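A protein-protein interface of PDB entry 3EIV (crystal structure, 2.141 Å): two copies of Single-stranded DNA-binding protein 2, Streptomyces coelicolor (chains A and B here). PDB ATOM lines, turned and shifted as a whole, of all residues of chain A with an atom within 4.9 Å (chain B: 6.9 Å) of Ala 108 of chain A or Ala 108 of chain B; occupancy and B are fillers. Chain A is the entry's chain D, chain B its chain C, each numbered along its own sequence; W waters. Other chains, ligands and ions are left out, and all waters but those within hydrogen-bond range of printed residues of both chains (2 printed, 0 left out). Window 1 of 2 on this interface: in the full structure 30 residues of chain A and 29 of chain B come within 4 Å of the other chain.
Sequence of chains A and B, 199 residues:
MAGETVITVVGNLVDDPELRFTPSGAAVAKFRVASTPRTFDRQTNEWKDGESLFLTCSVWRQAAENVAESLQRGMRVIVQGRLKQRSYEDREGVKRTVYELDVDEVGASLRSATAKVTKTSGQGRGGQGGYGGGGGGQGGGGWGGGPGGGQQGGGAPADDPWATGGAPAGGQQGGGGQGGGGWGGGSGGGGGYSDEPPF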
ATOM      1  N   LEU A  71       8.767 -26.455  27.741  1.00  0.00           N
ATOM      2  CA  LEU A  71       9.254 -26.423  26.364  1.00  0.00           C
ATOM      3  C   LEU A  71       9.404 -27.811  25.737  1.00  0.00           C
ATOM      4  O   LEU A  71       9.592 -28.811  26.438  1.00  0.00           O
ATOM      5  CB  LEU A  71      10.595 -25.676  26.289  1.00  0.00           C
ATOM      6  CG  LEU A  71      10.586 -24.210  26.749  1.00  0.00           C
ATOM      7  CD1 LEU A  71      11.942 -23.532  26.532  1.00  0.00           C
ATOM      8  CD2 LEU A  71       9.480 -23.439  26.043  1.00  0.00           C
ATOM      9  N   ARG A  76       9.462 -22.043  19.840  1.00  0.00           N
ATOM     10  CA  ARG A  76      10.330 -20.914  19.548  1.00  0.00           C
ATOM     11  C   ARG A  76      10.714 -20.214  20.847  1.00  0.00           C
ATOM     12  O   ARG A  76       9.857 -19.933  21.685  1.00  0.00           O
ATOM     13  CB  ARG A  76       9.621 -19.962  18.572  1.00  0.00           C
ATOM     14  CG  ARG A  76      10.502 -18.838  18.026  1.00  0.00           C
ATOM     15  CD  ARG A  76       9.658 -17.861  17.233  1.00  0.00           C
ATOM     16  NE  ARG A  76      10.409 -16.692  16.786  1.00  0.00           N
ATOM     17  CZ  ARG A  76      11.153 -16.659  15.682  1.00  0.00           C
ATOM     18  NH1 ARG A  76      11.265 -17.743  14.924  1.00  0.00           N
ATOM     19  NH2 ARG A  76      11.796 -15.550  15.339  1.00  0.00           N
ATOM     20  N   VAL A  77      12.008 -19.972  21.038  1.00  0.00           N
ATOM     21  CA  VAL A  77      12.493 -19.337  22.258  1.00  0.00           C
ATOM     22  C   VAL A  77      13.383 -18.149  21.969  1.00  0.00           C
ATOM     23  O   VAL A  77      13.945 -18.018  20.877  1.00  0.00           O
ATOM     24  CB  VAL A  77      13.351 -20.297  23.124  1.00  0.00           C
ATOM     25  CG1 VAL A  77      12.480 -21.331  23.834  1.00  0.00           C
ATOM     26  CG2 VAL A  77      14.450 -20.936  22.282  1.00  0.00           C
ATOM     27  N   VAL A 106      15.741 -17.256  29.690  1.00  0.00           N
ATOM     28  CA  VAL A 106      15.047 -17.912  28.578  1.00  0.00           C
ATOM     29  C   VAL A 106      13.554 -17.591  28.557  1.00  0.00           C
ATOM     30  O   VAL A 106      12.871 -17.687  29.572  1.00  0.00           O
ATOM     31  CB  VAL A 106      15.271 -19.446  28.565  1.00  0.00           C
ATOM     32  CG1 VAL A 106      14.943 -20.030  29.898  1.00  0.00           C
ATOM     33  CG2 VAL A 106      14.431 -20.110  27.462  1.00  0.00           C
ATOM     34  N   GLY A 107      13.048 -17.191  27.399  1.00  0.00           N
ATOM     35  CA  GLY A 107      11.627 -16.912  27.277  1.00  0.00           C
ATOM     36  C   GLY A 107      10.950 -17.705  26.172  1.00  0.00           C
ATOM     37  O   GLY A 107      11.554 -17.978  25.127  1.00  0.00           O
ATOM     38  N   ALA A 108       9.695 -18.083  26.396  1.00  0.00           N
ATOM     39  CA  ALA A 108       8.883 -18.653  25.319  1.00  0.00           C
ATOM     40  C   ALA A 108       8.418 -17.515  24.419  1.00  0.00           C
ATOM     41  O   ALA A 108       7.716 -16.601  24.876  1.00  0.00           O
ATOM     42  CB  ALA A 108       7.691 -19.413  25.881  1.00  0.00           C
ATOM     43  N   SER A 109       8.817 -17.556  23.149  1.00  0.00           N
ATOM     44  CA  SER A 109       8.490 -16.481  22.219  1.00  0.00           C
ATOM     45  C   SER A 109       7.001 -16.370  21.913  1.00  0.00           C
ATOM     46  O   SER A 109       6.323 -17.377  21.706  1.00  0.00           O
ATOM     47  CB  SER A 109       9.253 -16.648  20.902  1.00  0.00           C
ATOM     48  OG  SER A 109       8.876 -15.620  20.008  1.00  0.00           O
ATOM     49  N   LEU A 110       6.512 -15.133  21.866  1.00  0.00           N
ATOM     50  CA  LEU A 110       5.124 -14.832  21.524  1.00  0.00           C
ATOM     51  C   LEU A 110       4.976 -14.373  20.063  1.00  0.00           C
ATOM     52  O   LEU A 110       3.932 -13.852  19.653  1.00  0.00           O
ATOM     53  CB  LEU A 110       4.588 -13.759  22.471  1.00  0.00           C
ATOM     54  CG  LEU A 110       4.705 -14.054  23.977  1.00  0.00           C
ATOM     55  CD1 LEU A 110       4.041 -12.952  24.784  1.00  0.00           C
ATOM     56  CD2 LEU A 110       4.112 -15.417  24.326  1.00  0.00           C
ATOM     57  N   VAL A 117       0.646 -18.112  31.376  1.00  0.00           N
ATOM     58  CA  VAL A 117       1.793 -18.050  32.270  1.00  0.00           C
ATOM     59  C   VAL A 117       1.376 -18.216  33.728  1.00  0.00           C
ATOM     60  O   VAL A 117       0.487 -17.512  34.206  1.00  0.00           O
ATOM     61  CB  VAL A 117       2.527 -16.713  32.084  1.00  0.00           C
ATOM     62  CG1 VAL A 117       3.674 -16.561  33.090  1.00  0.00           C
ATOM     63  CG2 VAL A 117       3.024 -16.586  30.643  1.00  0.00           C
ATOM     64  N   SER B  70      -1.483 -12.690  26.365  1.00  0.00           N
ATOM     65  CA  SER B  70      -0.664 -13.528  27.250  1.00  0.00           C
ATOM     66  C   SER B  70      -0.096 -12.815  28.481  1.00  0.00           C
ATOM     67  O   SER B  70       0.008 -13.412  29.549  1.00  0.00           O
ATOM     68  CB  SER B  70       0.505 -14.137  26.477  1.00  0.00           C
ATOM     69  OG  SER B  70       0.079 -14.763  25.284  1.00  0.00           O
ATOM     70  N   LEU B  71       0.299 -11.556  28.321  1.00  0.00           N
ATOM     71  CA  LEU B  71       1.054 -10.851  29.363  1.00  0.00           C
ATOM     72  C   LEU B  71       0.209  -9.874  30.169  1.00  0.00           C
ATOM     73  O   LEU B  71      -0.702  -9.229  29.642  1.00  0.00           O
ATOM     74  CB  LEU B  71       2.242 -10.114  28.744  1.00  0.00           C
ATOM     75  CG  LEU B  71       3.189 -11.025  27.962  1.00  0.00           C
ATOM     76  CD1 LEU B  71       4.325 -10.243  27.316  1.00  0.00           C
ATOM     77  CD2 LEU B  71       3.732 -12.099  28.878  1.00  0.00           C
ATOM     78  N   MET B  75       4.353  -9.409  35.120  1.00  0.00           N
ATOM     79  CA  MET B  75       4.989 -10.578  34.528  1.00  0.00           C
ATOM     80  C   MET B  75       6.384 -10.258  34.023  1.00  0.00           C
ATOM     81  O   MET B  75       6.657  -9.143  33.576  1.00  0.00           O
ATOM     82  CB  MET B  75       4.148 -11.158  33.391  1.00  0.00           C
ATOM     83  CG  MET B  75       2.859 -11.826  33.842  1.00  0.00           C
ATOM     84  SD  MET B  75       1.986 -12.678  32.504  1.00  0.00           S
ATOM     85  CE  MET B  75       0.765 -13.599  33.442  1.00  0.00           C
ATOM     86  N   ARG B  76       7.260 -11.256  34.082  1.00  0.00           N
ATOM     87  CA  ARG B  76       8.635 -11.094  33.660  1.00  0.00           C
ATOM     88  C   ARG B  76       8.804 -11.429  32.174  1.00  0.00           C
ATOM     89  O   ARG B  76       8.329 -12.467  31.705  1.00  0.00           O
ATOM     90  CB  ARG B  76       9.537 -11.988  34.513  1.00  0.00           C
ATOM     91  CG  ARG B  76      11.019 -11.800  34.282  1.00  0.00           C
ATOM     92  CD  ARG B  76      11.806 -12.769  35.168  1.00  0.00           C
ATOM     93  NE  ARG B  76      13.244 -12.724  34.929  1.00  0.00           N
ATOM     94  CZ  ARG B  76      14.077 -11.896  35.555  1.00  0.00           C
ATOM     95  NH1 ARG B  76      13.610 -11.032  36.453  1.00  0.00           N
ATOM     96  NH2 ARG B  76      15.373 -11.933  35.287  1.00  0.00           N
ATOM     97  N   VAL B  77       9.500 -10.559  31.444  1.00  0.00           N
ATOM     98  CA  VAL B  77       9.729 -10.770  30.022  1.00  0.00           C
ATOM     99  C   VAL B  77      11.169 -10.558  29.592  1.00  0.00           C
ATOM    100  O   VAL B  77      11.952  -9.904  30.272  1.00  0.00           O
ATOM    101  CB  VAL B  77       8.870  -9.813  29.162  1.00  0.00           C
ATOM    102  CG1 VAL B  77       7.395 -10.139  29.331  1.00  0.00           C
ATOM    103  CG2 VAL B  77       9.176  -8.348  29.531  1.00  0.00           C
ATOM    104  N   ILE B  78      11.499 -11.117  28.438  1.00  0.00           N
ATOM    105  CA  ILE B  78      12.743 -10.815  27.754  1.00  0.00           C
ATOM    106  C   ILE B  78      12.409 -10.305  26.346  1.00  0.00           C
ATOM    107  O   ILE B  78      11.689 -10.958  25.586  1.00  0.00           O
ATOM    108  CB  ILE B  78      13.672 -12.051  27.692  1.00  0.00           C
ATOM    109  CG1 ILE B  78      14.878 -11.788  26.784  1.00  0.00           C
ATOM    110  CG2 ILE B  78      12.902 -13.289  27.231  1.00  0.00           C
ATOM    111  CD1 ILE B  78      15.996 -12.829  26.951  1.00  0.00           C
ATOM    112  N   VAL B 106       9.669 -10.810  21.620  1.00  0.00           N
ATOM    113  CA  VAL B 106       9.332 -10.783  23.029  1.00  0.00           C
ATOM    114  C   VAL B 106       8.993 -12.201  23.479  1.00  0.00           C
ATOM    115  O   VAL B 106       8.309 -12.940  22.767  1.00  0.00           O
ATOM    116  CB  VAL B 106       8.157  -9.823  23.321  1.00  0.00           C
ATOM    117  CG1 VAL B 106       7.015 -10.046  22.336  1.00  0.00           C
ATOM    118  CG2 VAL B 106       7.680  -9.954  24.777  1.00  0.00           C
ATOM    119  N   GLY B 107       9.526 -12.594  24.635  1.00  0.00           N
ATOM    120  CA  GLY B 107       9.226 -13.889  25.224  1.00  0.00           C
ATOM    121  C   GLY B 107       8.783 -13.746  26.664  1.00  0.00           C
ATOM    122  O   GLY B 107       9.244 -12.849  27.377  1.00  0.00           O
ATOM    123  N   ALA B 108       7.868 -14.611  27.088  1.00  0.00           N
ATOM    124  CA  ALA B 108       7.544 -14.736  28.502  1.00  0.00           C
ATOM    125  C   ALA B 108       8.671 -15.527  29.178  1.00  0.00           C
ATOM    126  O   ALA B 108       8.967 -16.665  28.799  1.00  0.00           O
ATOM    127  CB  ALA B 108       6.205 -15.432  28.679  1.00  0.00           C
ATOM    128  N   SER B 109       9.312 -14.919  30.167  1.00  0.00           N
ATOM    129  CA  SER B 109      10.455 -15.548  30.820  1.00  0.00           C
ATOM    130  C   SER B 109      10.045 -16.748  31.669  1.00  0.00           C
ATOM    131  O   SER B 109       9.010 -16.722  32.345  1.00  0.00           O
ATOM    132  CB  SER B 109      11.185 -14.545  31.712  1.00  0.00           C
ATOM    133  OG  SER B 109      12.212 -15.203  32.414  1.00  0.00           O
ATOM    134  N   LEU B 110      10.881 -17.779  31.659  1.00  0.00           N
ATOM    135  CA  LEU B 110      10.616 -18.986  32.430  1.00  0.00           C
ATOM    136  C   LEU B 110      11.482 -19.043  33.690  1.00  0.00           C
ATOM    137  O   LEU B 110      11.555 -20.074  34.364  1.00  0.00           O
ATOM    138  CB  LEU B 110      10.828 -20.233  31.553  1.00  0.00           C
ATOM    139  CG  LEU B 110       9.922 -20.287  30.314  1.00  0.00           C
ATOM    140  CD1 LEU B 110      10.157 -21.557  29.484  1.00  0.00           C
ATOM    141  CD2 LEU B 110       8.456 -20.181  30.717  1.00  0.00           C
ATOM    142  N   ARG B 111      12.139 -17.933  34.012  1.00  0.00           N
ATOM    143  CA  ARG B 111      12.997 -17.893  35.190  1.00  0.00           C
ATOM    144  C   ARG B 111      12.260 -18.363  36.448  1.00  0.00           C
ATOM    145  O   ARG B 111      12.799 -19.133  37.252  1.00  0.00           O
ATOM    146  CB  ARG B 111      13.573 -16.492  35.439  1.00  0.00           C
ATOM    147  CG  ARG B 111      14.301 -16.406  36.802  1.00  0.00           C
ATOM    148  CD  ARG B 111      15.016 -15.076  37.013  1.00  0.00           C
ATOM    149  NE  ARG B 111      16.077 -14.878  36.028  1.00  0.00           N
ATOM    150  CZ  ARG B 111      17.365 -15.104  36.261  1.00  0.00           C
ATOM    151  NH1 ARG B 111      17.761 -15.528  37.456  1.00  0.00           N
ATOM    152  NH2 ARG B 111      18.259 -14.902  35.300  1.00  0.00           N
ATOM    153  N   ALA B 113       8.523 -19.016  36.252  1.00  0.00           N
ATOM    154  CA  ALA B 113       7.175 -19.320  35.810  1.00  0.00           C
ATOM    155  C   ALA B 113       7.226 -20.468  34.812  1.00  0.00           C
ATOM    156  O   ALA B 113       8.276 -20.746  34.221  1.00  0.00           O
ATOM    157  CB  ALA B 113       6.519 -18.088  35.174  1.00  0.00           C
ATOM    158  N   ALA B 115       4.762 -22.132  31.486  1.00  0.00           N
ATOM    159  CA  ALA B 115       3.787 -21.632  30.539  1.00  0.00           C
ATOM    160  C   ALA B 115       3.184 -22.772  29.745  1.00  0.00           C
ATOM    161  O   ALA B 115       3.873 -23.744  29.430  1.00  0.00           O
ATOM    162  CB  ALA B 115       4.440 -20.626  29.597  1.00  0.00           C
ATOM    163  N   VAL B 117       2.000 -23.249  26.134  1.00  0.00           N
ATOM    164  CA  VAL B 117       2.200 -22.562  24.860  1.00  0.00           C
ATOM    165  C   VAL B 117       1.279 -23.126  23.782  1.00  0.00           C
ATOM    166  O   VAL B 117       1.093 -24.338  23.685  1.00  0.00           O
ATOM    167  CB  VAL B 117       3.673 -22.636  24.407  1.00  0.00           C
ATOM    168  CG1 VAL B 117       3.867 -21.916  23.075  1.00  0.00           C
ATOM    169  CG2 VAL B 117       4.590 -22.027  25.483  1.00  0.00           C
HETATM  170  O   HOH W   1      -0.780 -15.793  30.873  1.00  0.00           O
HETATM  171  O   HOH W   2      14.981 -17.647  32.419  1.00  0.00           O
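The backbone carbonyl oxygen of Ile 78 of chain B is in hydrogen-bond range of the backbone NH of Gly 107 of chain B, at 2.9 Å.
O of Arg 76 of chain B is in hydrogen-bond range of N of Ser 109 of chain B (3.1 Å).
O of Arg 76 of chain A is in hydrogen-bond range of N of Ser 109 of chain A (3.0 Å).
The side-chain hydroxyl (OG) of Ser 109 of chain B sits at hydrogen-bond distance from the backbone NH (N) of Arg 111 of chain B.
Hydrophobic or aromatic side chains of chain B within 4 Å of the printed part of chain A: Leu 71, Met 75, Ile 78, Ala 108, Leu 110 and Ala 113.
Of the 9 printed residues of chain A, 7 touch a printed residue of chain B.
Hydrophobic or aromatic side chains of chain A that line the printed part of chain B: Leu 71, Leu 110 and Val 117.
Val 106 of chain A touches Leu 110 of chain B, and with the chains exchanged Leu 110 of chain A touches Val 106 of chain B.
Gly 107 of chain A touches Ala 108 of chain B, and with the chains exchanged Ala 108 of chain A touches Gly 107 of chain B.
Ala 108 of chain A touches its own counterpart, Ala 108 of chain B.
Val 117 of chain A touches Ala 108 of chain B, but with the chains exchanged Ala 108 of chain A does not touch Val 117 of chain B (4.1 Å).
Positions printed for both chains: 71, 76, 77, 106, 107, 108, 109, 110 and 117.
Of the 14 pairs that touch across the chains among the printed residues, 9 have their exchanged pair printed and touching as well.
Printed residues of chain B within 4 Å of Leu 71 of chain A: Leu 110 (3.8 Å).
Arg 76 of chain A touches none of the printed residues of chain B.
Ala 108 of chain A touches two residues of chain B.
Of the printed residues of chain B, Ser 109 of chain A touches Val 106.
Arg 76 of chain B touches none of the printed residues of chain A.
Ala 108 of chain B touches just these residues of chain A: Gly 107, Ala 108 and Val 117.
The nearest residue of chain B that does not touch Ala 108 of chain A is Val 117 of chain B (4.1 Å).
Water W1 lies within hydrogen-bond range of N of Val 117 of chain A (2.8 Å) and O of Ser 70 of chain B (2.8 Å).
Water W2 lies within hydrogen-bond range of N of Val 106 of chain A (2.9 Å) and N of Arg 111 of chain B (3.3 Å).
Among the printed residues, pairs that only touch across the chains: Leu 71 of chain A with Leu 110 of chain B, Val 106 of chain A with Ser 109 of chain B, Gly 107 of chain A with Ile 78 of chain B, Gly 107 of chain A with Ala 108 of chain B, Gly 107 of chain A with Ser 109 of chain B, Ala 108 of chain A with Gly 107 of chain B, Ser 109 of chain A with Val 106 of chain B, Leu 110 of chain A with Leu 71 of chain B, Val 117 of chain A with Met 75 of chain B, Val 117 of chain A with Ala 108 of chain B and Val 117 of chain A with Ala 113 of chain B.
The backbone carbonyl oxygen of Val 106 of chain B is in hydrogen-bond range of the backbone NH of Leu 110 of chain A.
The backbone NH (N) of Leu 110 of chain B sits at hydrogen-bond distance from the backbone carbonyl oxygen (O) of Val 106 of chain A (2.9 Å).
The backbone NH of Ala 108 of chain A lies within hydrogen-bond range of the backbone carbonyl oxygen of Ala 108 of chain B, 2.9 Å away.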
